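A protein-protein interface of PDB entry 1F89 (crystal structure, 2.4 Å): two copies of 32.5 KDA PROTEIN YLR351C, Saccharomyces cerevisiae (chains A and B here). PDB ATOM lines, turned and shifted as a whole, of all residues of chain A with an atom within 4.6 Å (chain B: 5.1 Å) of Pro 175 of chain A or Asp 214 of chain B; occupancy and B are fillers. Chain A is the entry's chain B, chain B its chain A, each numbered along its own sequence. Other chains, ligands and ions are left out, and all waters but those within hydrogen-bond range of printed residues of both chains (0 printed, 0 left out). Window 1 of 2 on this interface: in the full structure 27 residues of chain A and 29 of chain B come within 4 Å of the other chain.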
ATOM      1  N   ARG A 173     -28.816 -21.161  32.034  1.00  0.00           N
ATOM      2  CA  ARG A 173     -27.923 -21.739  31.050  1.00  0.00           C
ATOM      3  C   ARG A 173     -28.685 -22.542  29.954  1.00  0.00           C
ATOM      4  O   ARG A 173     -28.078 -23.120  29.056  1.00  0.00           O
ATOM      5  CB  ARG A 173     -26.898 -22.597  31.778  1.00  0.00           C
ATOM      6  CG  ARG A 173     -25.503 -22.002  31.697  1.00  0.00           C
ATOM      7  CD  ARG A 173     -24.664 -22.260  32.938  1.00  0.00           C
ATOM      8  NE  ARG A 173     -23.284 -21.786  32.808  1.00  0.00           N
ATOM      9  CZ  ARG A 173     -22.459 -21.602  33.838  1.00  0.00           C
ATOM     10  NH1 ARG A 173     -22.864 -21.848  35.076  1.00  0.00           N
ATOM     11  NH2 ARG A 173     -21.219 -21.168  33.631  1.00  0.00           N
ATOM     12  N   PHE A 174     -30.016 -22.507  29.980  1.00  0.00           N
ATOM     13  CA  PHE A 174     -30.828 -23.296  29.042  1.00  0.00           C
ATOM     14  C   PHE A 174     -31.824 -22.309  28.513  1.00  0.00           C
ATOM     15  O   PHE A 174     -32.823 -22.000  29.182  1.00  0.00           O
ATOM     16  CB  PHE A 174     -31.542 -24.468  29.766  1.00  0.00           C
ATOM     17  CG  PHE A 174     -30.583 -25.484  30.396  1.00  0.00           C
ATOM     18  CD1 PHE A 174     -29.917 -25.162  31.562  1.00  0.00           C
ATOM     19  CD2 PHE A 174     -30.278 -26.693  29.771  1.00  0.00           C
ATOM     20  CE1 PHE A 174     -28.968 -25.984  32.099  1.00  0.00           C
ATOM     21  CE2 PHE A 174     -29.320 -27.540  30.296  1.00  0.00           C
ATOM     22  CZ  PHE A 174     -28.658 -27.181  31.470  1.00  0.00           C
ATOM     23  N   PRO A 175     -31.539 -21.774  27.320  1.00  0.00           N
ATOM     24  CA  PRO A 175     -32.397 -20.787  26.682  1.00  0.00           C
ATOM     25  C   PRO A 175     -33.854 -21.152  26.522  1.00  0.00           C
ATOM     26  O   PRO A 175     -34.696 -20.271  26.328  1.00  0.00           O
ATOM     27  CB  PRO A 175     -31.694 -20.535  25.354  1.00  0.00           C
ATOM     28  CG  PRO A 175     -31.084 -21.824  25.038  1.00  0.00           C
ATOM     29  CD  PRO A 175     -30.497 -22.248  26.390  1.00  0.00           C
ATOM     30  N   GLU A 176     -34.149 -22.444  26.575  1.00  0.00           N
ATOM     31  CA  GLU A 176     -35.517 -22.889  26.428  1.00  0.00           C
ATOM     32  C   GLU A 176     -36.417 -22.173  27.427  1.00  0.00           C
ATOM     33  O   GLU A 176     -37.420 -21.586  27.041  1.00  0.00           O
ATOM     34  CB  GLU A 176     -35.600 -24.403  26.612  1.00  0.00           C
ATOM     35  CG  GLU A 176     -35.252 -25.182  25.345  1.00  0.00           C
ATOM     36  CD  GLU A 176     -33.764 -25.261  25.082  1.00  0.00           C
ATOM     37  OE1 GLU A 176     -33.009 -24.480  25.692  1.00  0.00           O
ATOM     38  OE2 GLU A 176     -33.348 -26.103  24.255  1.00  0.00           O
ATOM     39  N   LEU A 177     -36.041 -22.206  28.703  1.00  0.00           N
ATOM     40  CA  LEU A 177     -36.815 -21.557  29.760  1.00  0.00           C
ATOM     41  C   LEU A 177     -37.153 -20.109  29.438  1.00  0.00           C
ATOM     42  O   LEU A 177     -38.261 -19.650  29.705  1.00  0.00           O
ATOM     43  CB  LEU A 177     -36.052 -21.619  31.083  1.00  0.00           C
ATOM     44  CG  LEU A 177     -36.219 -22.874  31.946  1.00  0.00           C
ATOM     45  CD1 LEU A 177     -36.044 -24.136  31.113  1.00  0.00           C
ATOM     46  CD2 LEU A 177     -35.209 -22.823  33.087  1.00  0.00           C
ATOM     47  N   ALA A 178     -36.202 -19.387  28.860  1.00  0.00           N
ATOM     48  CA  ALA A 178     -36.438 -17.988  28.522  1.00  0.00           C
ATOM     49  C   ALA A 178     -37.362 -17.865  27.325  1.00  0.00           C
ATOM     50  O   ALA A 178     -38.347 -17.140  27.376  1.00  0.00           O
ATOM     51  CB  ALA A 178     -35.118 -17.280  28.238  1.00  0.00           C
ATOM     52  N   MET A 179     -37.033 -18.575  26.244  1.00  0.00           N
ATOM     53  CA  MET A 179     -37.834 -18.541  25.023  1.00  0.00           C
ATOM     54  C   MET A 179     -39.289 -18.829  25.355  1.00  0.00           C
ATOM     55  O   MET A 179     -40.202 -18.166  24.866  1.00  0.00           O
ATOM     56  CB  MET A 179     -37.320 -19.585  24.028  1.00  0.00           C
ATOM     57  CG  MET A 179     -35.907 -19.334  23.501  1.00  0.00           C
ATOM     58  SD  MET A 179     -35.334 -20.701  22.482  1.00  0.00           S
ATOM     59  CE  MET A 179     -34.074 -21.293  23.393  1.00  0.00           C
ATOM     60  N   LEU A 207     -24.744 -14.310  29.759  1.00  0.00           N
ATOM     61  CA  LEU A 207     -26.043 -14.954  29.790  1.00  0.00           C
ATOM     62  C   LEU A 207     -27.151 -13.935  29.999  1.00  0.00           C
ATOM     63  O   LEU A 207     -28.134 -13.930  29.252  1.00  0.00           O
ATOM     64  CB  LEU A 207     -26.077 -16.015  30.886  1.00  0.00           C
ATOM     65  CG  LEU A 207     -25.041 -17.124  30.698  1.00  0.00           C
ATOM     66  CD1 LEU A 207     -24.833 -17.905  32.003  1.00  0.00           C
ATOM     67  CD2 LEU A 207     -25.497 -18.033  29.574  1.00  0.00           C
ATOM     68  N   ARG A 211     -29.933 -13.678  27.012  1.00  0.00           N
ATOM     69  CA  ARG A 211     -31.337 -14.039  27.158  1.00  0.00           C
ATOM     70  C   ARG A 211     -32.273 -12.848  26.896  1.00  0.00           C
ATOM     71  O   ARG A 211     -33.433 -13.031  26.511  1.00  0.00           O
ATOM     72  CB  ARG A 211     -31.576 -14.588  28.561  1.00  0.00           C
ATOM     73  CG  ARG A 211     -30.851 -15.896  28.851  1.00  0.00           C
ATOM     74  CD  ARG A 211     -31.486 -17.083  28.128  1.00  0.00           C
ATOM     75  NE  ARG A 211     -30.639 -18.270  28.192  1.00  0.00           N
ATOM     76  CZ  ARG A 211     -29.569 -18.457  27.427  1.00  0.00           C
ATOM     77  NH1 ARG A 211     -29.229 -17.537  26.537  1.00  0.00           N
ATOM     78  NH2 ARG A 211     -28.836 -19.554  27.558  1.00  0.00           N
ATOM     79  N   MET B 179     -28.703 -24.214  17.748  1.00  0.00           N
ATOM     80  CA  MET B 179     -29.080 -25.367  18.534  1.00  0.00           C
ATOM     81  C   MET B 179     -29.208 -26.574  17.610  1.00  0.00           C
ATOM     82  O   MET B 179     -28.712 -27.657  17.902  1.00  0.00           O
ATOM     83  CB  MET B 179     -30.407 -25.088  19.236  1.00  0.00           C
ATOM     84  CG  MET B 179     -30.338 -23.971  20.272  1.00  0.00           C
ATOM     85  SD  MET B 179     -31.922 -23.624  21.071  1.00  0.00           S
ATOM     86  CE  MET B 179     -32.429 -22.259  20.218  1.00  0.00           C
ATOM     87  N   ARG B 209     -20.342 -14.921  20.970  1.00  0.00           N
ATOM     88  CA  ARG B 209     -20.078 -15.598  22.242  1.00  0.00           C
ATOM     89  C   ARG B 209     -21.300 -16.277  22.858  1.00  0.00           C
ATOM     90  O   ARG B 209     -21.172 -17.242  23.613  1.00  0.00           O
ATOM     91  CB  ARG B 209     -19.496 -14.605  23.235  1.00  0.00           C
ATOM     92  CG  ARG B 209     -18.299 -13.852  22.691  1.00  0.00           C
ATOM     93  CD  ARG B 209     -17.798 -12.880  23.718  1.00  0.00           C
ATOM     94  NE  ARG B 209     -17.586 -13.583  24.976  1.00  0.00           N
ATOM     95  CZ  ARG B 209     -17.953 -13.121  26.164  1.00  0.00           C
ATOM     96  NH1 ARG B 209     -18.548 -11.945  26.248  1.00  0.00           N
ATOM     97  NH2 ARG B 209     -17.759 -13.854  27.252  1.00  0.00           N
ATOM     98  N   SER B 210     -22.484 -15.772  22.543  1.00  0.00           N
ATOM     99  CA  SER B 210     -23.699 -16.354  23.085  1.00  0.00           C
ATOM    100  C   SER B 210     -24.023 -17.704  22.443  1.00  0.00           C
ATOM    101  O   SER B 210     -24.389 -18.648  23.132  1.00  0.00           O
ATOM    102  CB  SER B 210     -24.870 -15.394  22.889  1.00  0.00           C
ATOM    103  OG  SER B 210     -26.094 -16.067  23.117  1.00  0.00           O
ATOM    104  N   ARG B 211     -23.888 -17.789  21.123  1.00  0.00           N
ATOM    105  CA  ARG B 211     -24.165 -19.024  20.389  1.00  0.00           C
ATOM    106  C   ARG B 211     -23.135 -20.114  20.670  1.00  0.00           C
ATOM    107  O   ARG B 211     -23.410 -21.294  20.484  1.00  0.00           O
ATOM    108  CB  ARG B 211     -24.201 -18.740  18.882  1.00  0.00           C
ATOM    109  CG  ARG B 211     -25.324 -17.810  18.442  1.00  0.00           C
ATOM    110  CD  ARG B 211     -26.669 -18.501  18.513  1.00  0.00           C
ATOM    111  NE  ARG B 211     -27.782 -17.564  18.410  1.00  0.00           N
ATOM    112  CZ  ARG B 211     -28.233 -16.832  19.422  1.00  0.00           C
ATOM    113  NH1 ARG B 211     -27.664 -16.931  20.615  1.00  0.00           N
ATOM    114  NH2 ARG B 211     -29.262 -16.013  19.248  1.00  0.00           N
ATOM    115  N   ALA B 212     -21.954 -19.708  21.129  1.00  0.00           N
ATOM    116  CA  ALA B 212     -20.860 -20.628  21.434  1.00  0.00           C
ATOM    117  C   ALA B 212     -20.970 -21.251  22.814  1.00  0.00           C
ATOM    118  O   ALA B 212     -20.693 -22.434  22.994  1.00  0.00           O
ATOM    119  CB  ALA B 212     -19.529 -19.905  21.317  1.00  0.00           C
ATOM    120  N   VAL B 213     -21.354 -20.446  23.792  1.00  0.00           N
ATOM    121  CA  VAL B 213     -21.492 -20.920  25.161  1.00  0.00           C
ATOM    122  C   VAL B 213     -22.811 -21.663  25.359  1.00  0.00           C
ATOM    123  O   VAL B 213     -22.895 -22.598  26.146  1.00  0.00           O
ATOM    124  CB  VAL B 213     -21.406 -19.737  26.149  1.00  0.00           C
ATOM    125  CG1 VAL B 213     -21.781 -20.186  27.550  1.00  0.00           C
ATOM    126  CG2 VAL B 213     -20.003 -19.176  26.134  1.00  0.00           C
ATOM    127  N   ASP B 214     -23.848 -21.244  24.648  1.00  0.00           N
ATOM    128  CA  ASP B 214     -25.138 -21.906  24.769  1.00  0.00           C
ATOM    129  C   ASP B 214     -25.104 -23.287  24.137  1.00  0.00           C
ATOM    130  O   ASP B 214     -25.735 -24.218  24.636  1.00  0.00           O
ATOM    131  CB  ASP B 214     -26.244 -21.077  24.116  1.00  0.00           C
ATOM    132  CG  ASP B 214     -27.002 -20.243  25.115  1.00  0.00           C
ATOM    133  OD1 ASP B 214     -28.169 -19.897  24.829  1.00  0.00           O
ATOM    134  OD2 ASP B 214     -26.428 -19.932  26.185  1.00  0.00           O
ATOM    135  N   ASN B 215     -24.380 -23.421  23.031  1.00  0.00           N
ATOM    136  CA  ASN B 215     -24.284 -24.718  22.370  1.00  0.00           C
ATOM    137  C   ASN B 215     -22.934 -25.392  22.647  1.00  0.00           C
ATOM    138  O   ASN B 215     -22.725 -26.535  22.265  1.00  0.00           O
ATOM    139  CB  ASN B 215     -24.497 -24.556  20.860  1.00  0.00           C
ATOM    140  CG  ASN B 215     -25.765 -23.784  20.533  1.00  0.00           C
ATOM    141  OD1 ASN B 215     -25.783 -22.558  20.573  1.00  0.00           O
ATOM    142  ND2 ASN B 215     -26.837 -24.502  20.225  1.00  0.00           N
ATOM    143  N   GLN B 216     -22.041 -24.679  23.335  1.00  0.00           N
ATOM    144  CA  GLN B 216     -20.697 -25.161  23.663  1.00  0.00           C
ATOM    145  C   GLN B 216     -20.006 -25.699  22.415  1.00  0.00           C
ATOM    146  O   GLN B 216     -19.502 -26.821  22.401  1.00  0.00           O
ATOM    147  CB  GLN B 216     -20.749 -26.245  24.749  1.00  0.00           C
ATOM    148  CG  GLN B 216     -21.640 -25.881  25.926  1.00  0.00           C
ATOM    149  CD  GLN B 216     -21.664 -26.944  27.012  1.00  0.00           C
ATOM    150  OE1 GLN B 216     -20.716 -27.081  27.782  1.00  0.00           O
ATOM    151  NE2 GLN B 216     -22.754 -27.702  27.078  1.00  0.00           N
ATOM    152  N   LYS B 278     -29.860 -31.597  29.291  1.00  0.00           N
ATOM    153  CA  LYS B 278     -31.003 -30.739  29.547  1.00  0.00           C
ATOM    154  C   LYS B 278     -32.243 -31.553  29.889  1.00  0.00           C
ATOM    155  O   LYS B 278     -32.415 -32.659  29.383  1.00  0.00           O
ATOM    156  CB  LYS B 278     -31.255 -29.898  28.292  1.00  0.00           C
ATOM    157  CG  LYS B 278     -29.949 -29.422  27.628  1.00  0.00           C
ATOM    158  CD  LYS B 278     -30.149 -28.901  26.200  1.00  0.00           C
ATOM    159  CE  LYS B 278     -28.852 -28.395  25.565  1.00  0.00           C
ATOM    160  NZ  LYS B 278     -28.396 -27.088  26.124  1.00  0.00           N
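The side-chain carboxylate (OD2) of Asp 214 of chain B lies within salt-bridge range of the guanidinium group (NH2) of Arg 211 of chain A (2.8 Å).
The backbone NH (N) of Met 179 of chain B lies close to the side-chain amide nitrogen (ND2) of Asn 215 of chain B (3.1 Å).
Phe 174 of chain A touches Lys 278 of chain B.
Asp 214 of chain B touches Pro 175 of chain A (OD1 to CG, 3.5 Å).
Met 179 of chain A touches Met 179 of chain B (CE to CE, 3.7 Å).
Leu 207 of chain A touches Asp 214 of chain B.
Arg 173 of chain A touches none of the printed residues of chain B.
Pro 175 of chain A touches just one residue of chain B: Asp 214 (3.5 Å).
Of the printed residues of chain B, Leu 207 of chain A touches Asp 214.
Ser 210 of chain B touches none of the printed residues of chain A.
Of the printed residues of chain A, Lys 278 of chain B touches Phe 174 (3.3 Å).
The nearest printed residue of chain A that does not touch Asp 214 of chain B is Arg 173 of chain A (4.6 Å).
Of the 9 printed residues of chain A, 5 touch a printed residue of chain B.
Hydrophobic or aromatic side chains of chain A within 4 Å of the printed part of chain B: Phe 174, Pro 175, Met 179 and Leu 207.
Met 179 of chain A touches its own counterpart, Met 179 of chain B.
Positions printed for both chains: 179 and 211.
Of the 5 pairs that touch across the chains among the printed residues, 1 has its exchanged pair printed and touching as well.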
